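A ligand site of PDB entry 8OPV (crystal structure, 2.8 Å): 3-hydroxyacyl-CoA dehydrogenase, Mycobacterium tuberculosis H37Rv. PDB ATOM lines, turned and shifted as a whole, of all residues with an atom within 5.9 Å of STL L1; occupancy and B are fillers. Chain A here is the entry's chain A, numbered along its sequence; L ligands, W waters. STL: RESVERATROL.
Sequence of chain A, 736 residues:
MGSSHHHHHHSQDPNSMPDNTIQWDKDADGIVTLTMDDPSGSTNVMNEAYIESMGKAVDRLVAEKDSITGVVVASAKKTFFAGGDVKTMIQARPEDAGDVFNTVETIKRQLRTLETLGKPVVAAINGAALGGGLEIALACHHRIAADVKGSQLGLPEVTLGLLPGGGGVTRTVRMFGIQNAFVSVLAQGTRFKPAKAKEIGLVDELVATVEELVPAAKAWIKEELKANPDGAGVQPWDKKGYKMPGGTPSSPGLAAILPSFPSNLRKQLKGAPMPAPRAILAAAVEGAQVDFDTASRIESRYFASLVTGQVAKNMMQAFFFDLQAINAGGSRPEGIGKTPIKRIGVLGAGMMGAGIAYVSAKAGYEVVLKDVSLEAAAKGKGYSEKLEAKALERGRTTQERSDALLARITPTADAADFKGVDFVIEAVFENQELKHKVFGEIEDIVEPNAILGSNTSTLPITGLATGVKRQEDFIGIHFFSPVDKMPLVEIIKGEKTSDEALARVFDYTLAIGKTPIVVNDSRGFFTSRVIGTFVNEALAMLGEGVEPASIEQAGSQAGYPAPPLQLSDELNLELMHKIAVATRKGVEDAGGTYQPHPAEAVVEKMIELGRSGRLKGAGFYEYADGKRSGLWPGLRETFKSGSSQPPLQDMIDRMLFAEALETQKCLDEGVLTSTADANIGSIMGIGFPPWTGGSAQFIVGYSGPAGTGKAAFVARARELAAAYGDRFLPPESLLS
Water W1 lies within hydrogen-bond range of the side-chain carboxylate of Glu 157 (3.0 Å) and an oxygen (O3) of STL L2 (3.1 Å).
O1 of STL L1 lies within hydrogen-bond range of OE2 of Glu 157 (2.5 Å).
An oxygen (O1) of STL L1 lies within hydrogen-bond range of the side-chain carboxylate of Glu 135.
OE1 of Glu 48 lies within hydrogen-bond range of O2 of STL L1, at 3.0 Å.
The backbone NH of Gly 132 lies within hydrogen-bond range of an oxygen (O1) of STL L1, at 3.4 Å.
O of Met 46 touches C4 of STL L1 (3.2 Å).
Asn 47 touches STL L1.
Thr 88 touches STL L1 (CG2 to C2, 3.9 Å).
Met 89 touches STL L1 (SD to C8, 3.7 Å).
Gly 131 touches STL L1 (C to O1, 3.7 Å).
Phe 303 touches STL L1 (CZ to C10, 3.6 Å).
Hydrophobic or aromatic side chains that line STL L1: Met 46, Met 89 and Phe 303.
Ten residues have an atom within 4 Å of STL L1: Met 46, Asn 47, Glu 48, Thr 88, Met 89, Gly 131, Gly 132, Glu 135, Glu 157 and Phe 303.
The backbone NH (N) of Leu 162 is in hydrogen-bond range of the backbone carbonyl oxygen (O) of Glu 157.
OE2 of Glu 135 sits at hydrogen-bond distance from N of Gly 166, 2.7 Å away.
OE2 of Glu 135 is in hydrogen-bond range of N of Gly 165 (3.3 Å).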
ATOM      1  N   MET A  46       5.332   6.254 -15.347  1.00  0.00           N
ATOM      2  CA  MET A  46       4.781   4.899 -15.372  1.00  0.00           C
ATOM      3  C   MET A  46       5.939   3.899 -15.371  1.00  0.00           C
ATOM      4  O   MET A  46       6.342   3.362 -16.407  1.00  0.00           O
ATOM      5  CB  MET A  46       3.875   4.719 -16.582  1.00  0.00           C
ATOM      6  CG  MET A  46       2.946   3.533 -16.482  1.00  0.00           C
ATOM      7  SD  MET A  46       1.400   3.822 -17.359  1.00  0.00           S
ATOM      8  CE  MET A  46       0.730   5.184 -16.417  1.00  0.00           C
ATOM      9  N   ASN A  47       6.473   3.667 -14.184  1.00  0.00           N
ATOM     10  CA  ASN A  47       7.584   2.743 -13.982  1.00  0.00           C
ATOM     11  C   ASN A  47       7.123   1.562 -13.128  1.00  0.00           C
ATOM     12  O   ASN A  47       5.920   1.374 -12.885  1.00  0.00           O
ATOM     13  CB  ASN A  47       8.769   3.476 -13.345  1.00  0.00           C
ATOM     14  CG  ASN A  47       8.379   4.283 -12.114  1.00  0.00           C
ATOM     15  OD1 ASN A  47       7.312   4.081 -11.544  1.00  0.00           O
ATOM     16  ND2 ASN A  47       9.257   5.195 -11.714  1.00  0.00           N
ATOM     17  N   GLU A  48       8.083   0.753 -12.678  1.00  0.00           N
ATOM     18  CA  GLU A  48       7.743  -0.437 -11.900  1.00  0.00           C
ATOM     19  C   GLU A  48       7.158  -0.085 -10.545  1.00  0.00           C
ATOM     20  O   GLU A  48       6.333  -0.841 -10.013  1.00  0.00           O
ATOM     21  CB  GLU A  48       8.982  -1.315 -11.721  1.00  0.00           C
ATOM     22  CG  GLU A  48       8.727  -2.804 -11.890  1.00  0.00           C
ATOM     23  CD  GLU A  48       8.416  -3.183 -13.325  1.00  0.00           C
ATOM     24  OE1 GLU A  48       8.831  -2.460 -14.241  1.00  0.00           O
ATOM     25  OE2 GLU A  48       7.739  -4.214 -13.535  1.00  0.00           O
ATOM     26  N   ILE A  51       3.307   0.752 -11.005  1.00  0.00           N
ATOM     27  CA  ILE A  51       2.474  -0.415 -11.300  1.00  0.00           C
ATOM     28  C   ILE A  51       2.155  -1.179 -10.027  1.00  0.00           C
ATOM     29  O   ILE A  51       1.005  -1.602  -9.817  1.00  0.00           O
ATOM     30  CB  ILE A  51       3.172  -1.304 -12.345  1.00  0.00           C
ATOM     31  CG1 ILE A  51       3.407  -0.528 -13.643  1.00  0.00           C
ATOM     32  CG2 ILE A  51       2.348  -2.553 -12.616  1.00  0.00           C
ATOM     33  CD1 ILE A  51       4.130  -1.317 -14.699  1.00  0.00           C
ATOM     34  N   GLY A  84       6.701   7.806 -19.078  1.00  0.00           N
ATOM     35  CA  GLY A  84       7.048   6.525 -18.507  1.00  0.00           C
ATOM     36  C   GLY A  84       8.534   6.344 -18.304  1.00  0.00           C
ATOM     37  O   GLY A  84       9.283   7.321 -18.241  1.00  0.00           O
ATOM     38  N   ASP A  85       8.980   5.087 -18.215  1.00  0.00           N
ATOM     39  CA  ASP A  85      10.376   4.754 -17.974  1.00  0.00           C
ATOM     40  C   ASP A  85      11.067   4.500 -19.310  1.00  0.00           C
ATOM     41  O   ASP A  85      11.009   3.394 -19.851  1.00  0.00           O
ATOM     42  CB  ASP A  85      10.481   3.543 -17.045  1.00  0.00           C
ATOM     43  CG  ASP A  85      11.891   3.321 -16.528  1.00  0.00           C
ATOM     44  OD1 ASP A  85      12.759   4.189 -16.771  1.00  0.00           O
ATOM     45  OD2 ASP A  85      12.132   2.282 -15.878  1.00  0.00           O
ATOM     46  N   THR A  88      14.053   1.983 -19.379  1.00  0.00           N
ATOM     47  CA  THR A  88      13.669   0.579 -19.489  1.00  0.00           C
ATOM     48  C   THR A  88      13.161   0.233 -20.886  1.00  0.00           C
ATOM     49  O   THR A  88      13.492  -0.834 -21.417  1.00  0.00           O
ATOM     50  CB  THR A  88      12.601   0.239 -18.443  1.00  0.00           C
ATOM     51  OG1 THR A  88      13.118   0.500 -17.138  1.00  0.00           O
ATOM     52  CG2 THR A  88      12.199  -1.220 -18.544  1.00  0.00           C
ATOM     53  N   MET A  89      12.384   1.128 -21.495  1.00  0.00           N
ATOM     54  CA  MET A  89      11.792   0.833 -22.798  1.00  0.00           C
ATOM     55  C   MET A  89      12.840   0.810 -23.909  1.00  0.00           C
ATOM     56  O   MET A  89      12.704   0.050 -24.874  1.00  0.00           O
ATOM     57  CB  MET A  89      10.691   1.837 -23.128  1.00  0.00           C
ATOM     58  CG  MET A  89       9.419   1.646 -22.312  1.00  0.00           C
ATOM     59  SD  MET A  89       8.129   2.839 -22.726  1.00  0.00           S
ATOM     60  CE  MET A  89       8.860   4.360 -22.136  1.00  0.00           C
ATOM     61  N   ALA A  92      14.423  -2.640 -24.418  1.00  0.00           N
ATOM     62  CA  ALA A  92      13.555  -3.770 -24.759  1.00  0.00           C
ATOM     63  C   ALA A  92      14.028  -4.430 -26.045  1.00  0.00           C
ATOM     64  O   ALA A  92      13.886  -3.858 -27.140  1.00  0.00           O
ATOM     65  CB  ALA A  92      12.108  -3.295 -24.887  1.00  0.00           C
ATOM     66  N   ASP A  99       7.555  -9.751 -22.124  1.00  0.00           N
ATOM     67  CA  ASP A  99       7.503  -8.925 -20.920  1.00  0.00           C
ATOM     68  C   ASP A  99       6.821  -7.586 -21.188  1.00  0.00           C
ATOM     69  O   ASP A  99       6.030  -7.109 -20.371  1.00  0.00           O
ATOM     70  CB  ASP A  99       8.905  -8.708 -20.365  1.00  0.00           C
ATOM     71  CG  ASP A  99       9.583 -10.006 -19.964  1.00  0.00           C
ATOM     72  OD1 ASP A  99       8.874 -11.011 -19.734  1.00  0.00           O
ATOM     73  OD2 ASP A  99      10.830 -10.023 -19.876  1.00  0.00           O
ATOM     74  N   VAL A 100       7.119  -6.971 -22.335  1.00  0.00           N
ATOM     75  CA  VAL A 100       6.485  -5.700 -22.696  1.00  0.00           C
ATOM     76  C   VAL A 100       4.985  -5.875 -22.832  1.00  0.00           C
ATOM     77  O   VAL A 100       4.188  -5.094 -22.298  1.00  0.00           O
ATOM     78  CB  VAL A 100       7.116  -5.134 -23.974  1.00  0.00           C
ATOM     79  CG1 VAL A 100       6.397  -3.858 -24.403  1.00  0.00           C
ATOM     80  CG2 VAL A 100       8.595  -4.859 -23.770  1.00  0.00           C
ATOM     81  N   THR A 103       3.416  -6.281 -19.442  1.00  0.00           N
ATOM     82  CA  THR A 103       3.448  -5.093 -18.594  1.00  0.00           C
ATOM     83  C   THR A 103       2.283  -4.164 -18.916  1.00  0.00           C
ATOM     84  O   THR A 103       1.562  -3.729 -18.008  1.00  0.00           O
ATOM     85  CB  THR A 103       4.784  -4.361 -18.752  1.00  0.00           C
ATOM     86  OG1 THR A 103       5.849  -5.209 -18.298  1.00  0.00           O
ATOM     87  CG2 THR A 103       4.793  -3.074 -17.940  1.00  0.00           C
ATOM     88  N   VAL A 104       2.079  -3.844 -20.203  1.00  0.00           N
ATOM     89  CA  VAL A 104       0.983  -2.947 -20.566  1.00  0.00           C
ATOM     90  C   VAL A 104      -0.356  -3.627 -20.356  1.00  0.00           C
ATOM     91  O   VAL A 104      -1.361  -2.954 -20.085  1.00  0.00           O
ATOM     92  CB  VAL A 104       1.159  -2.453 -22.017  1.00  0.00           C
ATOM     93  CG1 VAL A 104       2.381  -1.575 -22.131  1.00  0.00           C
ATOM     94  CG2 VAL A 104       1.251  -3.638 -22.969  1.00  0.00           C
ATOM     95  N   ILE A 107      -0.867  -2.968 -16.760  1.00  0.00           N
ATOM     96  CA  ILE A 107      -1.196  -1.551 -16.579  1.00  0.00           C
ATOM     97  C   ILE A 107      -2.656  -1.296 -16.928  1.00  0.00           C
ATOM     98  O   ILE A 107      -3.370  -0.597 -16.195  1.00  0.00           O
ATOM     99  CB  ILE A 107      -0.241  -0.664 -17.407  1.00  0.00           C
ATOM    100  CG1 ILE A 107       1.179  -0.760 -16.856  1.00  0.00           C
ATOM    101  CG2 ILE A 107      -0.731   0.770 -17.420  1.00  0.00           C
ATOM    102  CD1 ILE A 107       2.191   0.027 -17.664  1.00  0.00           C
ATOM    103  N   GLY A 131       0.918  11.330 -22.067  1.00  0.00           N
ATOM    104  CA  GLY A 131       1.197   9.920 -22.215  1.00  0.00           C
ATOM    105  C   GLY A 131       0.388   9.050 -21.279  1.00  0.00           C
ATOM    106  O   GLY A 131      -0.848   9.064 -21.307  1.00  0.00           O
ATOM    107  N   GLY A 132       1.076   8.277 -20.431  1.00  0.00           N
ATOM    108  CA  GLY A 132       0.371   7.437 -19.477  1.00  0.00           C
ATOM    109  C   GLY A 132      -0.440   8.244 -18.491  1.00  0.00           C
ATOM    110  O   GLY A 132      -1.397   7.727 -17.906  1.00  0.00           O
ATOM    111  N   GLU A 135      -3.727   8.773 -20.018  1.00  0.00           N
ATOM    112  CA  GLU A 135      -4.359   7.453 -20.063  1.00  0.00           C
ATOM    113  C   GLU A 135      -4.988   7.089 -18.716  1.00  0.00           C
ATOM    114  O   GLU A 135      -6.048   6.459 -18.671  1.00  0.00           O
ATOM    115  CB  GLU A 135      -3.341   6.398 -20.492  1.00  0.00           C
ATOM    116  CG  GLU A 135      -2.912   6.524 -21.937  1.00  0.00           C
ATOM    117  CD  GLU A 135      -1.931   5.440 -22.349  1.00  0.00           C
ATOM    118  OE1 GLU A 135      -1.004   5.152 -21.555  1.00  0.00           O
ATOM    119  OE2 GLU A 135      -2.088   4.869 -23.445  1.00  0.00           O
ATOM    120  N   LEU A 155      -1.437  12.730 -25.817  1.00  0.00           N
ATOM    121  CA  LEU A 155      -0.840  11.402 -25.930  1.00  0.00           C
ATOM    122  C   LEU A 155       0.304  11.464 -26.942  1.00  0.00           C
ATOM    123  O   LEU A 155       0.136  11.074 -28.099  1.00  0.00           O
ATOM    124  CB  LEU A 155      -1.879  10.358 -26.336  1.00  0.00           C
ATOM    125  CG  LEU A 155      -3.085  10.170 -25.419  1.00  0.00           C
ATOM    126  CD1 LEU A 155      -4.088   9.194 -26.027  1.00  0.00           C
ATOM    127  CD2 LEU A 155      -2.656   9.709 -24.037  1.00  0.00           C
ATOM    128  N   GLU A 157       3.151   9.847 -27.469  1.00  0.00           N
ATOM    129  CA  GLU A 157       4.127   8.757 -27.606  1.00  0.00           C
ATOM    130  C   GLU A 157       4.529   8.507 -29.052  1.00  0.00           C
ATOM    131  O   GLU A 157       5.575   7.893 -29.290  1.00  0.00           O
ATOM    132  CB  GLU A 157       3.592   7.463 -26.988  1.00  0.00           C
ATOM    133  CG  GLU A 157       2.128   7.481 -26.621  1.00  0.00           C
ATOM    134  CD  GLU A 157       1.865   8.060 -25.257  1.00  0.00           C
ATOM    135  OE1 GLU A 157       1.100   9.037 -25.168  1.00  0.00           O
ATOM    136  OE2 GLU A 157       2.443   7.551 -24.274  1.00  0.00           O
ATOM    137  N   LEU A 162       6.488   5.498 -30.263  1.00  0.00           N
ATOM    138  CA  LEU A 162       5.620   4.565 -29.551  1.00  0.00           C
ATOM    139  C   LEU A 162       4.162   4.850 -29.902  1.00  0.00           C
ATOM    140  O   LEU A 162       3.858   5.618 -30.823  1.00  0.00           O
ATOM    141  CB  LEU A 162       5.888   4.661 -28.056  1.00  0.00           C
ATOM    142  CG  LEU A 162       7.349   4.597 -27.608  1.00  0.00           C
ATOM    143  CD1 LEU A 162       7.478   4.890 -26.131  1.00  0.00           C
ATOM    144  CD2 LEU A 162       7.953   3.238 -27.949  1.00  0.00           C
ATOM    145  N   LEU A 163       3.261   4.230 -29.159  1.00  0.00           N
ATOM    146  CA  LEU A 163       1.830   4.485 -29.256  1.00  0.00           C
ATOM    147  C   LEU A 163       1.248   4.437 -27.856  1.00  0.00           C
ATOM    148  O   LEU A 163       1.829   3.821 -26.957  1.00  0.00           O
ATOM    149  CB  LEU A 163       1.123   3.477 -30.170  1.00  0.00           C
ATOM    150  CG  LEU A 163       1.063   1.976 -29.865  1.00  0.00           C
ATOM    151  CD1 LEU A 163      -0.054   1.629 -28.886  1.00  0.00           C
ATOM    152  CD2 LEU A 163       0.891   1.175 -31.152  1.00  0.00           C
ATOM    153  N   PRO A 164       0.109   5.090 -27.633  1.00  0.00           N
ATOM    154  CA  PRO A 164      -0.554   5.009 -26.318  1.00  0.00           C
ATOM    155  C   PRO A 164      -0.979   3.584 -25.985  1.00  0.00           C
ATOM    156  O   PRO A 164      -2.054   3.129 -26.387  1.00  0.00           O
ATOM    157  CB  PRO A 164      -1.768   5.927 -26.468  1.00  0.00           C
ATOM    158  CG  PRO A 164      -1.389   6.876 -27.549  1.00  0.00           C
ATOM    159  CD  PRO A 164      -0.561   6.070 -28.510  1.00  0.00           C
ATOM    160  N   GLY A 165      -0.125   2.860 -25.260  1.00  0.00           N
ATOM    161  CA  GLY A 165      -0.362   1.466 -24.964  1.00  0.00           C
ATOM    162  C   GLY A 165      -1.054   1.198 -23.654  1.00  0.00           C
ATOM    163  O   GLY A 165      -1.248   0.041 -23.276  1.00  0.00           O
ATOM    164  N   GLY A 166      -1.427   2.260 -22.935  1.00  0.00           N
ATOM    165  CA  GLY A 166      -2.153   2.108 -21.685  1.00  0.00           C
ATOM    166  C   GLY A 166      -3.630   2.446 -21.842  1.00  0.00           C
ATOM    167  O   GLY A 166      -4.245   2.990 -20.930  1.00  0.00           O
ATOM    168  N   PHE A 303       1.790  -2.127 -29.532  1.00  0.00           N
ATOM    169  CA  PHE A 303       2.755  -1.410 -28.705  1.00  0.00           C
ATOM    170  C   PHE A 303       4.047  -2.198 -28.559  1.00  0.00           C
ATOM    171  O   PHE A 303       5.134  -1.632 -28.643  1.00  0.00           O
ATOM    172  CB  PHE A 303       2.140  -1.109 -27.336  1.00  0.00           C
ATOM    173  CG  PHE A 303       3.078  -0.405 -26.391  1.00  0.00           C
ATOM    174  CD1 PHE A 303       3.237   0.973 -26.455  1.00  0.00           C
ATOM    175  CD2 PHE A 303       3.783  -1.120 -25.437  1.00  0.00           C
ATOM    176  CE1 PHE A 303       4.088   1.615 -25.580  1.00  0.00           C
ATOM    177  CE2 PHE A 303       4.635  -0.472 -24.569  1.00  0.00           C
ATOM    178  CZ  PHE A 303       4.784   0.903 -24.635  1.00  0.00           C
ATOM    179  N   VAL A 307       8.076  -0.931 -29.413  1.00  0.00           N
ATOM    180  CA  VAL A 307       9.116  -0.760 -28.406  1.00  0.00           C
ATOM    181  C   VAL A 307      10.325  -1.630 -28.726  1.00  0.00           C
ATOM    182  O   VAL A 307      11.480  -1.214 -28.536  1.00  0.00           O
ATOM    183  CB  VAL A 307       8.563  -1.057 -26.999  1.00  0.00           C
ATOM    184  CG1 VAL A 307       9.625  -0.807 -25.944  1.00  0.00           C
ATOM    185  CG2 VAL A 307       7.338  -0.207 -26.731  1.00  0.00           C
HETATM  186  C1  STL L   1       7.794  -1.230 -19.852  1.00  0.00           C
HETATM  187  C2  STL L   1       8.331  -1.234 -18.576  1.00  0.00           C
HETATM  188  C3  STL L   1       7.996  -0.257 -17.697  1.00  0.00           C
HETATM  189  C4  STL L   1       7.112   0.760 -18.078  1.00  0.00           C
HETATM  190  C5  STL L   1       6.585   0.761 -19.344  1.00  0.00           C
HETATM  191  C6  STL L   1       6.923  -0.223 -20.229  1.00  0.00           C
HETATM  192  C7  STL L   1       5.594   1.895 -19.794  1.00  0.00           C
HETATM  193  C8  STL L   1       5.070   1.847 -20.997  1.00  0.00           C
HETATM  194  C9  STL L   1       4.105   2.916 -21.486  1.00  0.00           C
HETATM  195  C10 STL L   1       4.496   3.795 -22.457  1.00  0.00           C
HETATM  196  C11 STL L   1       3.623   4.776 -22.905  1.00  0.00           C
HETATM  197  C12 STL L   1       2.352   4.856 -22.360  1.00  0.00           C
HETATM  198  C13 STL L   1       1.961   3.971 -21.380  1.00  0.00           C
HETATM  199  C14 STL L   1       2.818   3.014 -20.938  1.00  0.00           C
HETATM  200  O1  STL L   1       1.505   5.810 -22.792  1.00  0.00           O
HETATM  201  O2  STL L   1       8.564  -0.272 -16.341  1.00  0.00           O
HETATM  202  O3  STL L   1       8.123  -2.192 -20.719  1.00  0.00           O
HETATM  203  C1  STL L   2       5.817  11.065 -23.763  1.00  0.00           C
HETATM  204  C2  STL L   2       5.547  11.504 -22.482  1.00  0.00           C
HETATM  205  C3  STL L   2       5.915  12.759 -22.094  1.00  0.00           C
HETATM  206  C4  STL L   2       6.569  13.601 -22.994  1.00  0.00           C
HETATM  207  C5  STL L   2       6.836  13.169 -24.269  1.00  0.00           C
HETATM  208  C6  STL L   2       6.458  11.911 -24.659  1.00  0.00           C
HETATM  209  C7  STL L   2       7.565  14.110 -25.286  1.00  0.00           C
HETATM  210  C8  STL L   2       8.540  13.665 -26.062  1.00  0.00           C
HETATM  211  C9  STL L   2       9.209  14.634 -27.028  1.00  0.00           C
HETATM  212  C10 STL L   2       9.120  14.421 -28.382  1.00  0.00           C
HETATM  213  C11 STL L   2       9.735  15.301 -29.249  1.00  0.00           C
HETATM  214  C12 STL L   2      10.430  16.392 -28.765  1.00  0.00           C
HETATM  215  C13 STL L   2      10.511  16.596 -27.406  1.00  0.00           C
HETATM  216  C14 STL L   2       9.911  15.735 -26.536  1.00  0.00           C
HETATM  217  O1  STL L   2      11.018  17.245 -29.615  1.00  0.00           O
HETATM  218  O2  STL L   2       5.625  13.220 -20.731  1.00  0.00           O
HETATM  219  O3  STL L   2       5.452   9.834 -24.146  1.00  0.00           O
HETATM  220  O   HOH W   1       4.432   7.741 -22.033  1.00  0.00           O
